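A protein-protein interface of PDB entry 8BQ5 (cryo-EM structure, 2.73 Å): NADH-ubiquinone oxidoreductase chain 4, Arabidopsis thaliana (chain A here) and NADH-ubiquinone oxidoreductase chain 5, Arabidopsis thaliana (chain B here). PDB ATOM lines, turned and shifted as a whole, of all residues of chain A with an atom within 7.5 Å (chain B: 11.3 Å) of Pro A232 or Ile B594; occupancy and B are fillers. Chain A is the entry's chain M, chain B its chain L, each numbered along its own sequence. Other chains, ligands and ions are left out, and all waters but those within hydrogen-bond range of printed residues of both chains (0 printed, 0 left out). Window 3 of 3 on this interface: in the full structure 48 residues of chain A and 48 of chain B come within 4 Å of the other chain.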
ATOM      1  N   TYR A 176     -30.445   6.183 -20.027  1.00  0.00           N
ATOM      2  CA  TYR A 176     -30.080   5.945 -18.633  1.00  0.00           C
ATOM      3  C   TYR A 176     -31.132   6.520 -17.693  1.00  0.00           C
ATOM      4  O   TYR A 176     -31.620   5.836 -16.772  1.00  0.00           O
ATOM      5  CB  TYR A 176     -28.714   6.568 -18.345  1.00  0.00           C
ATOM      6  CG  TYR A 176     -27.548   5.627 -18.489  1.00  0.00           C
ATOM      7  CD1 TYR A 176     -27.137   4.834 -17.428  1.00  0.00           C
ATOM      8  CD2 TYR A 176     -26.848   5.537 -19.685  1.00  0.00           C
ATOM      9  CE1 TYR A 176     -26.068   3.977 -17.553  1.00  0.00           C
ATOM     10  CE2 TYR A 176     -25.778   4.683 -19.819  1.00  0.00           C
ATOM     11  CZ  TYR A 176     -25.392   3.905 -18.750  1.00  0.00           C
ATOM     12  OH  TYR A 176     -24.326   3.050 -18.876  1.00  0.00           O
ATOM     13  N   ALA A 225     -29.561   6.461  -7.890  1.00  0.00           N
ATOM     14  CA  ALA A 225     -28.112   6.246  -8.115  1.00  0.00           C
ATOM     15  C   ALA A 225     -27.717   6.486  -9.577  1.00  0.00           C
ATOM     16  O   ALA A 225     -26.531   6.727  -9.808  1.00  0.00           O
ATOM     17  CB  ALA A 225     -27.714   4.868  -7.649  1.00  0.00           C
ATOM     18  N   PRO A 229     -24.311  10.993 -10.075  1.00  0.00           N
ATOM     19  CA  PRO A 229     -24.337   9.552 -10.377  1.00  0.00           C
ATOM     20  C   PRO A 229     -23.451   8.661  -9.488  1.00  0.00           C
ATOM     21  O   PRO A 229     -22.501   9.156  -8.918  1.00  0.00           O
ATOM     22  CB  PRO A 229     -23.750   9.538 -11.788  1.00  0.00           C
ATOM     23  CG  PRO A 229     -22.706  10.610 -11.758  1.00  0.00           C
ATOM     24  CD  PRO A 229     -23.329  11.692 -10.906  1.00  0.00           C
ATOM     25  N   MET A 230     -23.766   7.364  -9.417  1.00  0.00           N
ATOM     26  CA  MET A 230     -22.924   6.416  -8.635  1.00  0.00           C
ATOM     27  C   MET A 230     -22.278   5.381  -9.566  1.00  0.00           C
ATOM     28  O   MET A 230     -22.864   5.111 -10.618  1.00  0.00           O
ATOM     29  CB  MET A 230     -23.766   5.713  -7.568  1.00  0.00           C
ATOM     30  CG  MET A 230     -24.340   6.674  -6.548  1.00  0.00           C
ATOM     31  SD  MET A 230     -24.997   5.879  -5.067  1.00  0.00           S
ATOM     32  CE  MET A 230     -23.530   5.811  -4.042  1.00  0.00           C
ATOM     33  N   VAL A 231     -21.099   4.853  -9.209  1.00  0.00           N
ATOM     34  CA  VAL A 231     -20.426   3.831 -10.006  1.00  0.00           C
ATOM     35  C   VAL A 231     -21.254   2.552  -9.931  1.00  0.00           C
ATOM     36  O   VAL A 231     -21.803   2.236  -8.865  1.00  0.00           O
ATOM     37  CB  VAL A 231     -18.982   3.597  -9.530  1.00  0.00           C
ATOM     38  CG1 VAL A 231     -18.100   4.772  -9.918  1.00  0.00           C
ATOM     39  CG2 VAL A 231     -18.934   3.358  -8.025  1.00  0.00           C
ATOM     40  N   PRO A 232     -21.384   1.789 -11.023  1.00  0.00           N
ATOM     41  CA  PRO A 232     -20.837   2.022 -12.361  1.00  0.00           C
ATOM     42  C   PRO A 232     -21.851   2.575 -13.362  1.00  0.00           C
ATOM     43  O   PRO A 232     -21.731   2.309 -14.553  1.00  0.00           O
ATOM     44  CB  PRO A 232     -20.377   0.621 -12.764  1.00  0.00           C
ATOM     45  CG  PRO A 232     -21.437  -0.276 -12.165  1.00  0.00           C
ATOM     46  CD  PRO A 232     -21.941   0.430 -10.913  1.00  0.00           C
ATOM     47  N   VAL A 233     -22.854   3.342 -12.939  1.00  0.00           N
ATOM     48  CA  VAL A 233     -23.835   3.882 -13.875  1.00  0.00           C
ATOM     49  C   VAL A 233     -23.580   5.373 -14.051  1.00  0.00           C
ATOM     50  O   VAL A 233     -24.506   6.149 -14.314  1.00  0.00           O
ATOM     51  CB  VAL A 233     -25.280   3.607 -13.413  1.00  0.00           C
ATOM     52  CG1 VAL A 233     -25.625   2.135 -13.595  1.00  0.00           C
ATOM     53  CG2 VAL A 233     -25.487   4.035 -11.973  1.00  0.00           C
ATOM     54  N   HIS A 234     -22.322   5.780 -13.899  1.00  0.00           N
ATOM     55  CA  HIS A 234     -21.917   7.175 -14.006  1.00  0.00           C
ATOM     56  C   HIS A 234     -21.417   7.562 -15.393  1.00  0.00           C
ATOM     57  O   HIS A 234     -21.166   8.747 -15.631  1.00  0.00           O
ATOM     58  CB  HIS A 234     -20.812   7.466 -12.992  1.00  0.00           C
ATOM     59  CG  HIS A 234     -19.542   6.725 -13.268  1.00  0.00           C
ATOM     60  ND1 HIS A 234     -19.399   5.378 -13.016  1.00  0.00           N
ATOM     61  CD2 HIS A 234     -18.362   7.138 -13.786  1.00  0.00           C
ATOM     62  CE1 HIS A 234     -18.184   4.993 -13.365  1.00  0.00           C
ATOM     63  NE2 HIS A 234     -17.534   6.043 -13.832  1.00  0.00           N
ATOM     64  N   ILE A 235     -21.268   6.601 -16.310  1.00  0.00           N
ATOM     65  CA  ILE A 235     -20.566   6.858 -17.564  1.00  0.00           C
ATOM     66  C   ILE A 235     -21.387   7.669 -18.556  1.00  0.00           C
ATOM     67  O   ILE A 235     -20.836   8.163 -19.545  1.00  0.00           O
ATOM     68  CB  ILE A 235     -20.125   5.531 -18.199  1.00  0.00           C
ATOM     69  CG1 ILE A 235     -21.328   4.838 -18.839  1.00  0.00           C
ATOM     70  CG2 ILE A 235     -19.455   4.644 -17.164  1.00  0.00           C
ATOM     71  CD1 ILE A 235     -20.982   3.586 -19.568  1.00  0.00           C
ATOM     72  N   TRP A 236     -22.695   7.808 -18.342  1.00  0.00           N
ATOM     73  CA  TRP A 236     -23.477   8.685 -19.205  1.00  0.00           C
ATOM     74  C   TRP A 236     -23.141  10.150 -18.954  1.00  0.00           C
ATOM     75  O   TRP A 236     -23.224  10.971 -19.873  1.00  0.00           O
ATOM     76  CB  TRP A 236     -24.967   8.439 -18.990  1.00  0.00           C
ATOM     77  CG  TRP A 236     -25.430   8.846 -17.629  1.00  0.00           C
ATOM     78  CD1 TRP A 236     -25.576   8.039 -16.542  1.00  0.00           C
ATOM     79  CD2 TRP A 236     -25.820  10.159 -17.211  1.00  0.00           C
ATOM     80  NE1 TRP A 236     -26.021   8.768 -15.469  1.00  0.00           N
ATOM     81  CE2 TRP A 236     -26.180  10.073 -15.853  1.00  0.00           C
ATOM     82  CE3 TRP A 236     -25.899  11.399 -17.852  1.00  0.00           C
ATOM     83  CZ2 TRP A 236     -26.608  11.177 -15.126  1.00  0.00           C
ATOM     84  CZ3 TRP A 236     -26.319  12.495 -17.126  1.00  0.00           C
ATOM     85  CH2 TRP A 236     -26.672  12.376 -15.779  1.00  0.00           C
ATOM     86  N   LEU A 286     -19.600   2.205  -2.219  1.00  0.00           N
ATOM     87  CA  LEU A 286     -19.748   2.736  -3.569  1.00  0.00           C
ATOM     88  C   LEU A 286     -19.288   4.185  -3.638  1.00  0.00           C
ATOM     89  O   LEU A 286     -18.587   4.585  -4.574  1.00  0.00           O
ATOM     90  CB  LEU A 286     -21.203   2.625  -4.025  1.00  0.00           C
ATOM     91  CG  LEU A 286     -21.679   1.330  -4.678  1.00  0.00           C
ATOM     92  CD1 LEU A 286     -23.161   1.442  -4.997  1.00  0.00           C
ATOM     93  CD2 LEU A 286     -20.877   1.007  -5.924  1.00  0.00           C
ATOM     94  N   TYR A 293     -11.637   6.467  -7.429  1.00  0.00           N
ATOM     95  CA  TYR A 293     -11.457   6.053  -8.819  1.00  0.00           C
ATOM     96  C   TYR A 293     -11.669   7.216  -9.781  1.00  0.00           C
ATOM     97  O   TYR A 293     -10.855   7.441 -10.685  1.00  0.00           O
ATOM     98  CB  TYR A 293     -12.411   4.911  -9.169  1.00  0.00           C
ATOM     99  CG  TYR A 293     -11.980   3.538  -8.708  1.00  0.00           C
ATOM    100  CD1 TYR A 293     -11.067   3.377  -7.675  1.00  0.00           C
ATOM    101  CD2 TYR A 293     -12.494   2.400  -9.312  1.00  0.00           C
ATOM    102  CE1 TYR A 293     -10.683   2.120  -7.258  1.00  0.00           C
ATOM    103  CE2 TYR A 293     -12.116   1.144  -8.904  1.00  0.00           C
ATOM    104  CZ  TYR A 293     -11.212   1.007  -7.877  1.00  0.00           C
ATOM    105  OH  TYR A 293     -10.837  -0.250  -7.471  1.00  0.00           O
ATOM    106  N   PHE B 580      -2.605   4.425 -12.731  1.00  0.00           N
ATOM    107  CA  PHE B 580      -3.897   3.862 -12.356  1.00  0.00           C
ATOM    108  C   PHE B 580      -5.037   4.632 -13.009  1.00  0.00           C
ATOM    109  O   PHE B 580      -5.998   4.036 -13.510  1.00  0.00           O
ATOM    110  CB  PHE B 580      -4.048   3.861 -10.832  1.00  0.00           C
ATOM    111  CG  PHE B 580      -5.334   3.246 -10.344  1.00  0.00           C
ATOM    112  CD1 PHE B 580      -6.494   4.000 -10.260  1.00  0.00           C
ATOM    113  CD2 PHE B 580      -5.381   1.918  -9.962  1.00  0.00           C
ATOM    114  CE1 PHE B 580      -7.674   3.440  -9.810  1.00  0.00           C
ATOM    115  CE2 PHE B 580      -6.559   1.352  -9.512  1.00  0.00           C
ATOM    116  CZ  PHE B 580      -7.707   2.115  -9.436  1.00  0.00           C
ATOM    117  N   GLU B 583      -5.027   3.621 -17.021  1.00  0.00           N
ATOM    118  CA  GLU B 583      -5.049   2.226 -17.445  1.00  0.00           C
ATOM    119  C   GLU B 583      -6.076   1.380 -16.705  1.00  0.00           C
ATOM    120  O   GLU B 583      -6.421   0.298 -17.188  1.00  0.00           O
ATOM    121  CB  GLU B 583      -3.668   1.597 -17.274  1.00  0.00           C
ATOM    122  CG  GLU B 583      -2.609   2.170 -18.187  1.00  0.00           C
ATOM    123  CD  GLU B 583      -1.214   1.867 -17.697  1.00  0.00           C
ATOM    124  OE1 GLU B 583      -0.861   0.671 -17.633  1.00  0.00           O
ATOM    125  OE2 GLU B 583      -0.474   2.818 -17.372  1.00  0.00           O
ATOM    126  N   VAL B 584      -6.564   1.822 -15.550  1.00  0.00           N
ATOM    127  CA  VAL B 584      -7.455   0.966 -14.776  1.00  0.00           C
ATOM    128  C   VAL B 584      -8.823   1.610 -14.612  1.00  0.00           C
ATOM    129  O   VAL B 584      -9.829   1.082 -15.099  1.00  0.00           O
ATOM    130  CB  VAL B 584      -6.848   0.632 -13.402  1.00  0.00           C
ATOM    131  CG1 VAL B 584      -7.764  -0.310 -12.648  1.00  0.00           C
ATOM    132  CG2 VAL B 584      -5.468   0.022 -13.564  1.00  0.00           C
ATOM    133  N   SER B 585      -8.875   2.754 -13.930  1.00  0.00           N
ATOM    134  CA  SER B 585     -10.168   3.355 -13.621  1.00  0.00           C
ATOM    135  C   SER B 585     -10.858   3.858 -14.882  1.00  0.00           C
ATOM    136  O   SER B 585     -12.091   3.867 -14.963  1.00  0.00           O
ATOM    137  CB  SER B 585      -9.996   4.483 -12.602  1.00  0.00           C
ATOM    138  OG  SER B 585      -9.235   5.550 -13.135  1.00  0.00           O
ATOM    139  N   PHE B 586     -10.081   4.261 -15.886  1.00  0.00           N
ATOM    140  CA  PHE B 586     -10.633   4.768 -17.136  1.00  0.00           C
ATOM    141  C   PHE B 586     -10.682   3.703 -18.227  1.00  0.00           C
ATOM    142  O   PHE B 586     -11.749   3.429 -18.784  1.00  0.00           O
ATOM    143  CB  PHE B 586      -9.821   5.978 -17.612  1.00  0.00           C
ATOM    144  CG  PHE B 586     -10.357   6.607 -18.862  1.00  0.00           C
ATOM    145  CD1 PHE B 586     -11.648   7.106 -18.903  1.00  0.00           C
ATOM    146  CD2 PHE B 586      -9.573   6.696 -19.998  1.00  0.00           C
ATOM    147  CE1 PHE B 586     -12.143   7.683 -20.054  1.00  0.00           C
ATOM    148  CE2 PHE B 586     -10.064   7.271 -21.150  1.00  0.00           C
ATOM    149  CZ  PHE B 586     -11.349   7.767 -21.179  1.00  0.00           C
ATOM    150  N   GLU B 587      -9.539   3.095 -18.543  1.00  0.00           N
ATOM    151  CA  GLU B 587      -9.458   2.207 -19.698  1.00  0.00           C
ATOM    152  C   GLU B 587      -9.989   0.813 -19.381  1.00  0.00           C
ATOM    153  O   GLU B 587     -10.744   0.237 -20.171  1.00  0.00           O
ATOM    154  CB  GLU B 587      -8.013   2.137 -20.197  1.00  0.00           C
ATOM    155  CG  GLU B 587      -7.814   1.310 -21.451  1.00  0.00           C
ATOM    156  CD  GLU B 587      -6.432   1.486 -22.051  1.00  0.00           C
ATOM    157  OE1 GLU B 587      -5.436   1.380 -21.305  1.00  0.00           O
ATOM    158  OE2 GLU B 587      -6.342   1.738 -23.271  1.00  0.00           O
ATOM    159  N   ALA B 588      -9.601   0.249 -18.236  1.00  0.00           N
ATOM    160  CA  ALA B 588     -10.058  -1.094 -17.898  1.00  0.00           C
ATOM    161  C   ALA B 588     -11.515  -1.095 -17.452  1.00  0.00           C
ATOM    162  O   ALA B 588     -12.277  -2.000 -17.811  1.00  0.00           O
ATOM    163  CB  ALA B 588      -9.165  -1.704 -16.818  1.00  0.00           C
ATOM    164  N   LEU B 589     -11.922  -0.099 -16.667  1.00  0.00           N
ATOM    165  CA  LEU B 589     -13.271  -0.113 -16.117  1.00  0.00           C
ATOM    166  C   LEU B 589     -14.234   0.785 -16.884  1.00  0.00           C
ATOM    167  O   LEU B 589     -15.203   0.293 -17.466  1.00  0.00           O
ATOM    168  CB  LEU B 589     -13.242   0.293 -14.643  1.00  0.00           C
ATOM    169  CG  LEU B 589     -12.446  -0.642 -13.736  1.00  0.00           C
ATOM    170  CD1 LEU B 589     -12.177   0.001 -12.386  1.00  0.00           C
ATOM    171  CD2 LEU B 589     -13.191  -1.954 -13.572  1.00  0.00           C
ATOM    172  N   ASP B 590     -13.967   2.092 -16.918  1.00  0.00           N
ATOM    173  CA  ASP B 590     -14.923   3.022 -17.512  1.00  0.00           C
ATOM    174  C   ASP B 590     -15.090   2.759 -19.004  1.00  0.00           C
ATOM    175  O   ASP B 590     -16.164   2.359 -19.462  1.00  0.00           O
ATOM    176  CB  ASP B 590     -14.486   4.463 -17.248  1.00  0.00           C
ATOM    177  CG  ASP B 590     -15.047   5.008 -15.944  1.00  0.00           C
ATOM    178  OD1 ASP B 590     -15.403   4.195 -15.067  1.00  0.00           O
ATOM    179  OD2 ASP B 590     -15.128   6.244 -15.793  1.00  0.00           O
ATOM    180  N   LYS B 591     -14.026   2.941 -19.776  1.00  0.00           N
ATOM    181  CA  LYS B 591     -14.073   2.640 -21.199  1.00  0.00           C
ATOM    182  C   LYS B 591     -13.908   1.157 -21.490  1.00  0.00           C
ATOM    183  O   LYS B 591     -13.804   0.777 -22.660  1.00  0.00           O
ATOM    184  CB  LYS B 591     -13.002   3.435 -21.948  1.00  0.00           C
ATOM    185  CG  LYS B 591     -13.247   4.930 -21.959  1.00  0.00           C
ATOM    186  CD  LYS B 591     -14.672   5.246 -22.378  1.00  0.00           C
ATOM    187  CE  LYS B 591     -14.707   6.254 -23.512  1.00  0.00           C
ATOM    188  NZ  LYS B 591     -15.989   6.179 -24.264  1.00  0.00           N
ATOM    189  N   GLY B 592     -13.873   0.313 -20.462  1.00  0.00           N
ATOM    190  CA  GLY B 592     -13.686  -1.109 -20.659  1.00  0.00           C
ATOM    191  C   GLY B 592     -14.881  -1.952 -20.267  1.00  0.00           C
ATOM    192  O   GLY B 592     -15.869  -2.025 -21.002  1.00  0.00           O
ATOM    193  N   ALA B 593     -14.798  -2.585 -19.093  1.00  0.00           N
ATOM    194  CA  ALA B 593     -15.826  -3.534 -18.674  1.00  0.00           C
ATOM    195  C   ALA B 593     -17.188  -2.868 -18.540  1.00  0.00           C
ATOM    196  O   ALA B 593     -18.211  -3.452 -18.914  1.00  0.00           O
ATOM    197  CB  ALA B 593     -15.426  -4.192 -17.355  1.00  0.00           C
ATOM    198  N   ILE B 594     -17.227  -1.654 -17.992  1.00  0.00           N
ATOM    199  CA  ILE B 594     -18.503  -0.968 -17.820  1.00  0.00           C
ATOM    200  C   ILE B 594     -19.112  -0.631 -19.176  1.00  0.00           C
ATOM    201  O   ILE B 594     -20.338  -0.648 -19.343  1.00  0.00           O
ATOM    202  CB  ILE B 594     -18.320   0.275 -16.931  1.00  0.00           C
ATOM    203  CG1 ILE B 594     -17.710  -0.131 -15.588  1.00  0.00           C
ATOM    204  CG2 ILE B 594     -19.645   0.980 -16.709  1.00  0.00           C
ATOM    205  CD1 ILE B 594     -17.391   1.030 -14.679  1.00  0.00           C
ATOM    206  N   GLU B 595     -18.272  -0.321 -20.165  1.00  0.00           N
ATOM    207  CA  GLU B 595     -18.776  -0.128 -21.521  1.00  0.00           C
ATOM    208  C   GLU B 595     -19.246  -1.445 -22.135  1.00  0.00           C
ATOM    209  O   GLU B 595     -20.358  -1.521 -22.668  1.00  0.00           O
ATOM    210  CB  GLU B 595     -17.700   0.520 -22.391  1.00  0.00           C
ATOM    211  CG  GLU B 595     -17.759   2.046 -22.468  1.00  0.00           C
ATOM    212  CD  GLU B 595     -19.023   2.574 -23.126  1.00  0.00           C
ATOM    213  OE1 GLU B 595     -20.114   2.458 -22.533  1.00  0.00           O
ATOM    214  OE2 GLU B 595     -18.920   3.115 -24.246  1.00  0.00           O
ATOM    215  N   ILE B 596     -18.421  -2.494 -22.062  1.00  0.00           N
ATOM    216  CA  ILE B 596     -18.782  -3.760 -22.698  1.00  0.00           C
ATOM    217  C   ILE B 596     -19.973  -4.393 -21.986  1.00  0.00           C
ATOM    218  O   ILE B 596     -20.924  -4.854 -22.628  1.00  0.00           O
ATOM    219  CB  ILE B 596     -17.569  -4.710 -22.749  1.00  0.00           C
ATOM    220  CG1 ILE B 596     -16.848  -4.594 -24.094  1.00  0.00           C
ATOM    221  CG2 ILE B 596     -18.000  -6.155 -22.561  1.00  0.00           C
ATOM    222  CD1 ILE B 596     -16.477  -3.182 -24.490  1.00  0.00           C
ATOM    223  N   LEU B 597     -19.949  -4.418 -20.658  1.00  0.00           N
ATOM    224  CA  LEU B 597     -21.134  -4.778 -19.880  1.00  0.00           C
ATOM    225  C   LEU B 597     -22.020  -3.559 -19.657  1.00  0.00           C
ATOM    226  O   LEU B 597     -22.419  -3.243 -18.537  1.00  0.00           O
ATOM    227  CB  LEU B 597     -20.729  -5.407 -18.551  1.00  0.00           C
ATOM    228  CG  LEU B 597     -20.194  -6.838 -18.539  1.00  0.00           C
ATOM    229  CD1 LEU B 597     -18.704  -6.880 -18.836  1.00  0.00           C
ATOM    230  CD2 LEU B 597     -20.490  -7.477 -17.194  1.00  0.00           C
ATOM    231  N   GLY B 598     -22.334  -2.863 -20.743  1.00  0.00           N
ATOM    232  CA  GLY B 598     -23.102  -1.647 -20.669  1.00  0.00           C
ATOM    233  C   GLY B 598     -23.525  -1.160 -22.038  1.00  0.00           C
ATOM    234  O   GLY B 598     -23.831  -1.950 -22.934  1.00  0.00           O
ATOM    235  N   PRO B 599     -23.523   0.160 -22.228  1.00  0.00           N
ATOM    236  CA  PRO B 599     -24.111   0.723 -23.457  1.00  0.00           C
ATOM    237  C   PRO B 599     -23.452   0.242 -24.740  1.00  0.00           C
ATOM    238  O   PRO B 599     -24.143   0.092 -25.754  1.00  0.00           O
ATOM    239  CB  PRO B 599     -23.953   2.241 -23.274  1.00  0.00           C
ATOM    240  CG  PRO B 599     -23.355   2.456 -21.936  1.00  0.00           C
ATOM    241  CD  PRO B 599     -22.861   1.168 -21.388  1.00  0.00           C
ATOM    242  N   TYR B 600     -22.139   0.011 -24.740  1.00  0.00           N
ATOM    243  CA  TYR B 600     -21.499  -0.519 -25.939  1.00  0.00           C
ATOM    244  C   TYR B 600     -21.949  -1.948 -26.217  1.00  0.00           C
ATOM    245  O   TYR B 600     -22.354  -2.277 -27.337  1.00  0.00           O
ATOM    246  CB  TYR B 600     -19.979  -0.462 -25.804  1.00  0.00           C
ATOM    247  CG  TYR B 600     -19.259  -0.781 -27.092  1.00  0.00           C
ATOM    248  CD1 TYR B 600     -19.338   0.074 -28.182  1.00  0.00           C
ATOM    249  CD2 TYR B 600     -18.517  -1.946 -27.227  1.00  0.00           C
ATOM    250  CE1 TYR B 600     -18.687  -0.212 -29.362  1.00  0.00           C
ATOM    251  CE2 TYR B 600     -17.861  -2.243 -28.407  1.00  0.00           C
ATOM    252  CZ  TYR B 600     -17.951  -1.371 -29.472  1.00  0.00           C
ATOM    253  OH  TYR B 600     -17.305  -1.655 -30.651  1.00  0.00           O
ATOM    254  N   GLY B 601     -21.867  -2.813 -25.207  1.00  0.00           N
ATOM    255  CA  GLY B 601     -22.274  -4.195 -25.392  1.00  0.00           C
ATOM    256  C   GLY B 601     -23.771  -4.352 -25.568  1.00  0.00           C
ATOM    257  O   GLY B 601     -24.226  -5.183 -26.356  1.00  0.00           O
ATOM    258  N   ILE B 602     -24.557  -3.570 -24.822  1.00  0.00           N
ATOM    259  CA  ILE B 602     -26.012  -3.666 -24.907  1.00  0.00           C
ATOM    260  C   ILE B 602     -26.498  -3.250 -26.288  1.00  0.00           C
ATOM    261  O   ILE B 602     -27.397  -3.878 -26.862  1.00  0.00           O
ATOM    262  CB  ILE B 602     -26.667  -2.827 -23.794  1.00  0.00           C
ATOM    263  CG1 ILE B 602     -26.711  -3.620 -22.487  1.00  0.00           C
ATOM    264  CG2 ILE B 602     -28.059  -2.364 -24.204  1.00  0.00           C
ATOM    265  CD1 ILE B 602     -26.608  -2.763 -21.250  1.00  0.00           C
ATOM    266  N   SER B 603     -25.919  -2.184 -26.841  1.00  0.00           N
ATOM    267  CA  SER B 603     -26.315  -1.734 -28.172  1.00  0.00           C
ATOM    268  C   SER B 603     -26.014  -2.790 -29.229  1.00  0.00           C
ATOM    269  O   SER B 603     -26.832  -3.034 -30.125  1.00  0.00           O
ATOM    270  CB  SER B 603     -25.613  -0.418 -28.503  1.00  0.00           C
ATOM    271  OG  SER B 603     -24.391  -0.643 -29.181  1.00  0.00           O
ATOM    272  N   TYR B 604     -24.852  -3.438 -29.130  1.00  0.00           N
ATOM    273  CA  TYR B 604     -24.451  -4.433 -30.120  1.00  0.00           C
ATOM    274  C   TYR B 604     -25.408  -5.620 -30.138  1.00  0.00           C
ATOM    275  O   TYR B 604     -25.886  -6.036 -31.203  1.00  0.00           O
ATOM    276  CB  TYR B 604     -23.011  -4.880 -29.835  1.00  0.00           C
ATOM    277  CG  TYR B 604     -22.594  -6.210 -30.436  1.00  0.00           C
ATOM    278  CD1 TYR B 604     -22.895  -7.414 -29.805  1.00  0.00           C
ATOM    279  CD2 TYR B 604     -21.894  -6.259 -31.633  1.00  0.00           C
ATOM    280  CE1 TYR B 604     -22.516  -8.622 -30.353  1.00  0.00           C
ATOM    281  CE2 TYR B 604     -21.510  -7.465 -32.188  1.00  0.00           C
ATOM    282  CZ  TYR B 604     -21.824  -8.643 -31.544  1.00  0.00           C
ATOM    283  OH  TYR B 604     -21.443  -9.844 -32.091  1.00  0.00           O
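Hydrophobic or aromatic side chains of chain A that line the printed part of chain B: Tyr A176, Pro A232, His A234, Ile A235 and Tyr A293.
Along chain A the printed residues that touch a printed residue of chain B span positions 176 to 293.
Of chain B, only Ile B594 (3.3 Å) comes within 4 Å of Pro A232.
Of chain B, only Asp B590 comes within 4 Å of His A234.
Of the printed residues of chain B, Tyr A293 touches Phe B580 (3.7 Å), Ser B585 (3.5 Å) and Leu B589 (3.7 Å).
Of the printed residues of chain A, Phe B580 touches Tyr A293.
No residue of chain A comes within 4 Å of Ala B593.
Of chain A, only Pro A232 (3.3 Å) and Ile A235 (3.7 Å) come within 4 Å of Ile B594.
Of the printed residues of chain A, Glu B595 touches Ile A235 (3.3 Å).
Among the printed residues, pairs that only touch across the chains: Tyr A176 with Pro B599 (3.3 Å), Pro A232 with Ile B594 (3.3 Å), Ile A235 with Ile B594 (3.7 Å), Ile A235 with Glu B595 (3.3 Å), Ile A235 with Pro B599 (3.5 Å), Tyr A293 with Phe B580 (3.7 Å) and Tyr A293 with Leu B589 (3.7 Å).
The backbone carbonyl oxygen (O) of Phe B580 is in hydrogen-bond range of the backbone NH (N) of Ser B585.
N of Glu B595 sits close to O of Asp B590 (3.5 Å).
N of Leu B589 is in hydrogen-bond range of O of Val B584, at 2.9 Å.
O of Glu B595 is in hydrogen-bond range of N of Gly B601 (3.2 Å).
The backbone carbonyl oxygen (O) of Ser B585 lies within hydrogen-bond range of the backbone NH (N) of Asp B590 (3.2 Å).
The backbone NH (N) of Ile B594 lies within hydrogen-bond range of the backbone carbonyl oxygen (O) of Leu B589 (2.9 Å).
The side-chain carboxylate (OD1) of Asp B590 sits at hydrogen-bond distance from a ring nitrogen (NE2) of His A234 (3.1 Å).
The side-chain hydroxyl (OG) of Ser B585 lies within hydrogen-bond range of the backbone carbonyl oxygen (O) of Tyr A293 (3.5 Å).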
